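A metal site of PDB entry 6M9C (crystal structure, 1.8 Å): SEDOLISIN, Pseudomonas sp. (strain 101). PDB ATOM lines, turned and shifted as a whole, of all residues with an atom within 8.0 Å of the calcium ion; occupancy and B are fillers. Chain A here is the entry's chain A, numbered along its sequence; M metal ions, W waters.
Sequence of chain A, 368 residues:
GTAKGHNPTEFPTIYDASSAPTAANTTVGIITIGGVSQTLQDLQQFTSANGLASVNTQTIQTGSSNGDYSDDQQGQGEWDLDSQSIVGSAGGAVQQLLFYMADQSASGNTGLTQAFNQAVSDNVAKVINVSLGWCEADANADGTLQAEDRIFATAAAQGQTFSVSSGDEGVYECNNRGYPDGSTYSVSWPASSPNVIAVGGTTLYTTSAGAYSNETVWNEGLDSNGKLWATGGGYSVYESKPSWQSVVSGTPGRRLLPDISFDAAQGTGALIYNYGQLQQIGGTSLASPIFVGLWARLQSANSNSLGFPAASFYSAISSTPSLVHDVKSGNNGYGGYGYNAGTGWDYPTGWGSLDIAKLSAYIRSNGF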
ATOM      1  N   VAL A 217      26.378  -9.812 -28.385  1.00  0.00           N
ATOM      2  CA  VAL A 217      25.010 -10.191 -28.006  1.00  0.00           C
ATOM      3  C   VAL A 217      24.365 -10.848 -29.205  1.00  0.00           C
ATOM      4  O   VAL A 217      24.574 -10.386 -30.331  1.00  0.00           O
ATOM      5  CB  VAL A 217      24.212  -8.954 -27.578  1.00  0.00           C
ATOM      6  CG1 VAL A 217      22.752  -9.274 -27.276  1.00  0.00           C
ATOM      7  CG2 VAL A 217      24.871  -8.351 -26.347  1.00  0.00           C
ATOM      8  N   VAL A 324      35.543 -16.499 -17.764  1.00  0.00           N
ATOM      9  CA  VAL A 324      34.529 -16.284 -18.783  1.00  0.00           C
ATOM     10  C   VAL A 324      35.043 -15.462 -19.966  1.00  0.00           C
ATOM     11  O   VAL A 324      36.019 -14.716 -19.867  1.00  0.00           O
ATOM     12  CB  VAL A 324      33.271 -15.572 -18.223  1.00  0.00           C
ATOM     13  CG1 VAL A 324      32.531 -16.500 -17.271  1.00  0.00           C
ATOM     14  CG2 VAL A 324      33.654 -14.264 -17.541  1.00  0.00           C
ATOM     15  N   HIS A 325      34.333 -15.618 -21.077  1.00  0.00           N
ATOM     16  CA  HIS A 325      34.406 -14.670 -22.170  1.00  0.00           C
ATOM     17  C   HIS A 325      33.293 -13.640 -21.878  1.00  0.00           C
ATOM     18  O   HIS A 325      32.132 -13.986 -22.075  1.00  0.00           O
ATOM     19  CB  HIS A 325      34.200 -15.253 -23.552  1.00  0.00           C
ATOM     20  CG  HIS A 325      35.128 -16.380 -23.881  1.00  0.00           C
ATOM     21  ND1 HIS A 325      36.483 -16.147 -24.033  1.00  0.00           N
ATOM     22  CD2 HIS A 325      34.968 -17.704 -24.051  1.00  0.00           C
ATOM     23  CE1 HIS A 325      37.096 -17.292 -24.303  1.00  0.00           C
ATOM     24  NE2 HIS A 325      36.204 -18.262 -24.317  1.00  0.00           N
ATOM     25  N   ASP A 326      33.696 -12.459 -21.447  1.00  0.00           N
ATOM     26  CA  ASP A 326      32.769 -11.377 -21.124  1.00  0.00           C
ATOM     27  C   ASP A 326      32.234 -10.655 -22.343  1.00  0.00           C
ATOM     28  O   ASP A 326      32.965  -9.944 -23.048  1.00  0.00           O
ATOM     29  CB  ASP A 326      33.520 -10.397 -20.202  1.00  0.00           C
ATOM     30  CG  ASP A 326      32.633  -9.245 -19.761  1.00  0.00           C
ATOM     31  OD1 ASP A 326      31.394  -9.329 -19.906  1.00  0.00           O
ATOM     32  OD2 ASP A 326      33.227  -8.254 -19.276  1.00  0.00           O
ATOM     33  N   VAL A 327      30.956 -10.815 -22.648  1.00  0.00           N
ATOM     34  CA  VAL A 327      30.367 -10.147 -23.816  1.00  0.00           C
ATOM     35  C   VAL A 327      30.213  -8.683 -23.491  1.00  0.00           C
ATOM     36  O   VAL A 327      29.714  -8.312 -22.435  1.00  0.00           O
ATOM     37  CB  VAL A 327      29.023 -10.775 -24.175  1.00  0.00           C
ATOM     38  CG1 VAL A 327      28.311  -9.986 -25.260  1.00  0.00           C
ATOM     39  CG2 VAL A 327      29.223 -12.230 -24.593  1.00  0.00           C
ATOM     40  N   LYS A 328      30.642  -7.804 -24.385  1.00  0.00           N
ATOM     41  CA  LYS A 328      30.582  -6.378 -24.101  1.00  0.00           C
ATOM     42  C   LYS A 328      29.801  -5.555 -25.108  1.00  0.00           C
ATOM     43  O   LYS A 328      29.474  -4.410 -24.817  1.00  0.00           O
ATOM     44  CB  LYS A 328      32.011  -5.808 -24.046  1.00  0.00           C
ATOM     45  CG  LYS A 328      32.814  -6.295 -22.854  1.00  0.00           C
ATOM     46  CD  LYS A 328      34.254  -5.831 -22.916  1.00  0.00           C
ATOM     47  CE  LYS A 328      34.864  -5.683 -21.541  1.00  0.00           C
ATOM     48  NZ  LYS A 328      36.211  -6.320 -21.466  1.00  0.00           N
ATOM     49  N   SER A 329      29.508  -6.121 -26.279  1.00  0.00           N
ATOM     50  CA  SER A 329      28.880  -5.420 -27.367  1.00  0.00           C
ATOM     51  C   SER A 329      27.540  -5.986 -27.809  1.00  0.00           C
ATOM     52  O   SER A 329      27.423  -7.193 -28.072  1.00  0.00           O
ATOM     53  CB  SER A 329      29.861  -5.436 -28.576  1.00  0.00           C
ATOM     54  OG  SER A 329      29.198  -4.956 -29.734  1.00  0.00           O
ATOM     55  N   ASN A 340      21.746  -3.111 -22.724  1.00  0.00           N
ATOM     56  CA  ASN A 340      23.049  -3.147 -23.397  1.00  0.00           C
ATOM     57  C   ASN A 340      24.027  -4.047 -22.673  1.00  0.00           C
ATOM     58  O   ASN A 340      24.080  -4.099 -21.441  1.00  0.00           O
ATOM     59  CB  ASN A 340      23.654  -1.748 -23.473  1.00  0.00           C
ATOM     60  CG  ASN A 340      22.752  -0.768 -24.209  1.00  0.00           C
ATOM     61  OD1 ASN A 340      22.367  -0.975 -25.367  1.00  0.00           O
ATOM     62  ND2 ASN A 340      22.410   0.299 -23.502  1.00  0.00           N
ATOM     63  N   ALA A 341      24.833  -4.741 -23.464  1.00  0.00           N
ATOM     64  CA  ALA A 341      25.963  -5.456 -22.914  1.00  0.00           C
ATOM     65  C   ALA A 341      26.986  -4.457 -22.369  1.00  0.00           C
ATOM     66  O   ALA A 341      26.981  -3.303 -22.784  1.00  0.00           O
ATOM     67  CB  ALA A 341      26.624  -6.320 -23.979  1.00  0.00           C
ATOM     68  N   GLY A 342      27.842  -4.942 -21.500  1.00  0.00           N
ATOM     69  CA  GLY A 342      28.917  -4.146 -20.926  1.00  0.00           C
ATOM     70  C   GLY A 342      29.921  -4.990 -20.184  1.00  0.00           C
ATOM     71  O   GLY A 342      29.895  -6.208 -20.168  1.00  0.00           O
ATOM     72  N   THR A 343      30.858  -4.306 -19.535  1.00  0.00           N
ATOM     73  CA  THR A 343      31.842  -5.005 -18.733  1.00  0.00           C
ATOM     74  C   THR A 343      31.133  -5.749 -17.612  1.00  0.00           C
ATOM     75  O   THR A 343      30.271  -5.146 -16.971  1.00  0.00           O
ATOM     76  CB  THR A 343      32.905  -4.051 -18.158  1.00  0.00           C
ATOM     77  OG1 THR A 343      33.597  -3.466 -19.280  1.00  0.00           O
ATOM     78  CG2 THR A 343      33.912  -4.808 -17.302  1.00  0.00           C
ATOM     79  N   GLY A 344      31.483  -7.009 -17.400  1.00  0.00           N
ATOM     80  CA  GLY A 344      30.934  -7.784 -16.298  1.00  0.00           C
ATOM     81  C   GLY A 344      29.547  -8.313 -16.626  1.00  0.00           C
ATOM     82  O   GLY A 344      29.156  -8.502 -17.787  1.00  0.00           O
ATOM     83  N   TRP A 345      28.774  -8.596 -15.574  1.00  0.00           N
ATOM     84  CA  TRP A 345      27.444  -9.166 -15.771  1.00  0.00           C
ATOM     85  C   TRP A 345      26.584  -8.132 -16.472  1.00  0.00           C
ATOM     86  O   TRP A 345      26.602  -6.952 -16.100  1.00  0.00           O
ATOM     87  CB  TRP A 345      26.835  -9.559 -14.416  1.00  0.00           C
ATOM     88  CG  TRP A 345      25.567 -10.352 -14.536  1.00  0.00           C
ATOM     89  CD1 TRP A 345      25.484 -11.711 -14.403  1.00  0.00           C
ATOM     90  CD2 TRP A 345      24.250  -9.881 -14.803  1.00  0.00           C
ATOM     91  NE1 TRP A 345      24.182 -12.103 -14.574  1.00  0.00           N
ATOM     92  CE2 TRP A 345      23.411 -11.016 -14.822  1.00  0.00           C
ATOM     93  CE3 TRP A 345      23.680  -8.618 -15.027  1.00  0.00           C
ATOM     94  CZ2 TRP A 345      22.044 -10.904 -15.055  1.00  0.00           C
ATOM     95  CZ3 TRP A 345      22.327  -8.523 -15.264  1.00  0.00           C
ATOM     96  CH2 TRP A 345      21.531  -9.673 -15.273  1.00  0.00           C
ATOM     97  N   ASP A 346      25.811  -8.518 -17.472  1.00  0.00           N
ATOM     98  CA  ASP A 346      24.840  -7.623 -18.064  1.00  0.00           C
ATOM     99  C   ASP A 346      23.538  -8.364 -18.360  1.00  0.00           C
ATOM    100  O   ASP A 346      23.489  -9.599 -18.327  1.00  0.00           O
ATOM    101  CB  ASP A 346      25.383  -6.934 -19.323  1.00  0.00           C
ATOM    102  CG  ASP A 346      25.978  -7.921 -20.333  1.00  0.00           C
ATOM    103  OD1 ASP A 346      25.209  -8.800 -20.798  1.00  0.00           O
ATOM    104  OD2 ASP A 346      27.190  -7.788 -20.621  1.00  0.00           O
ATOM    105  N   TYR A 347      22.481  -7.611 -18.613  1.00  0.00           N
ATOM    106  CA  TYR A 347      21.172  -8.236 -18.800  1.00  0.00           C
ATOM    107  C   TYR A 347      21.091  -9.068 -20.076  1.00  0.00           C
ATOM    108  O   TYR A 347      20.426 -10.116 -20.028  1.00  0.00           O
ATOM    109  CB  TYR A 347      20.062  -7.198 -18.753  1.00  0.00           C
ATOM    110  CG  TYR A 347      19.738  -6.710 -17.361  1.00  0.00           C
ATOM    111  CD1 TYR A 347      19.114  -7.546 -16.437  1.00  0.00           C
ATOM    112  CD2 TYR A 347      20.054  -5.416 -16.966  1.00  0.00           C
ATOM    113  CE1 TYR A 347      18.810  -7.127 -15.161  1.00  0.00           C
ATOM    114  CE2 TYR A 347      19.734  -4.992 -15.691  1.00  0.00           C
ATOM    115  CZ  TYR A 347      19.123  -5.848 -14.785  1.00  0.00           C
ATOM    116  OH  TYR A 347      18.822  -5.375 -13.512  1.00  0.00           O
ATOM    117  N   PRO A 348      21.662  -8.691 -21.207  1.00  0.00           N
ATOM    118  CA  PRO A 348      21.535  -9.591 -22.357  1.00  0.00           C
ATOM    119  C   PRO A 348      22.204 -10.945 -22.178  1.00  0.00           C
ATOM    120  O   PRO A 348      21.674 -11.945 -22.660  1.00  0.00           O
ATOM    121  CB  PRO A 348      22.258  -8.798 -23.472  1.00  0.00           C
ATOM    122  CG  PRO A 348      22.071  -7.363 -23.071  1.00  0.00           C
ATOM    123  CD  PRO A 348      22.342  -7.428 -21.580  1.00  0.00           C
ATOM    124  N   THR A 349      23.354 -11.015 -21.520  1.00  0.00           N
ATOM    125  CA  THR A 349      24.154 -12.239 -21.598  1.00  0.00           C
ATOM    126  C   THR A 349      24.684 -12.771 -20.283  1.00  0.00           C
ATOM    127  O   THR A 349      25.398 -13.777 -20.187  1.00  0.00           O
ATOM    128  CB  THR A 349      25.399 -12.017 -22.520  1.00  0.00           C
ATOM    129  OG1 THR A 349      26.182 -10.946 -22.037  1.00  0.00           O
ATOM    130  CG2 THR A 349      24.903 -11.672 -23.915  1.00  0.00           C
ATOM    131  N   GLY A 350      24.332 -12.090 -19.192  1.00  0.00           N
ATOM    132  CA  GLY A 350      24.838 -12.494 -17.893  1.00  0.00           C
ATOM    133  C   GLY A 350      26.348 -12.373 -17.792  1.00  0.00           C
ATOM    134  O   GLY A 350      26.907 -11.336 -18.150  1.00  0.00           O
ATOM    135  N   TRP A 351      27.013 -13.413 -17.317  1.00  0.00           N
ATOM    136  CA  TRP A 351      28.470 -13.392 -17.184  1.00  0.00           C
ATOM    137  C   TRP A 351      29.186 -13.626 -18.512  1.00  0.00           C
ATOM    138  O   TRP A 351      30.407 -13.470 -18.581  1.00  0.00           O
ATOM    139  CB  TRP A 351      28.900 -14.426 -16.156  1.00  0.00           C
ATOM    140  CG  TRP A 351      28.597 -14.078 -14.738  1.00  0.00           C
ATOM    141  CD1 TRP A 351      27.763 -14.759 -13.905  1.00  0.00           C
ATOM    142  CD2 TRP A 351      29.093 -12.971 -13.968  1.00  0.00           C
ATOM    143  NE1 TRP A 351      27.708 -14.161 -12.683  1.00  0.00           N
ATOM    144  CE2 TRP A 351      28.512 -13.052 -12.675  1.00  0.00           C
ATOM    145  CE3 TRP A 351      29.963 -11.906 -14.208  1.00  0.00           C
ATOM    146  CZ2 TRP A 351      28.778 -12.137 -11.667  1.00  0.00           C
ATOM    147  CZ3 TRP A 351      30.230 -10.991 -13.201  1.00  0.00           C
ATOM    148  CH2 TRP A 351      29.635 -11.101 -11.924  1.00  0.00           C
ATOM    149  N   GLY A 352      28.417 -13.981 -19.531  1.00  0.00           N
ATOM    150  CA  GLY A 352      28.951 -14.375 -20.834  1.00  0.00           C
ATOM    151  C   GLY A 352      29.180 -15.869 -20.885  1.00  0.00           C
ATOM    152  O   GLY A 352      28.512 -16.608 -20.167  1.00  0.00           O
HETATM  153 CA    CA M   1      29.311  -8.463 -20.140  1.00  0.00          CA
HETATM  154  O   HOH W   1      28.445 -10.786 -20.265  1.00  0.00           O
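The side-chain carboxylate of Asp 346 lies within hydrogen-bond range of the side-chain hydroxyl of Thr 349 (2.7 Å).
Five residues have an atom within 4 Å of the calcium ion: Asp 326, Val 327, Gly 342, Gly 344 and Asp 346.
OD1 of Asp 326 binds the calcium ion (2.3 Å).
The calcium ion is bound by OD2 of Asp 346 (2.3 Å).
The backbone carbonyl oxygen (O) of Gly 342 binds the calcium ion.
The calcium ion is bound by O of Val 327, 2.3 Å away.
The calcium ion is bound by O of Gly 344, 2.4 Å away.
The calcium ion is bound by water W1 (2.5 Å).
The calcium ion has six donor atoms within binding distance.
Water W1 lies within hydrogen-bond range of O of Gly 350 (2.7 Å), OG1 of Thr 349 (2.9 Å), N of Gly 352 (3.3 Å) and N of Val 327 (3.5 Å).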
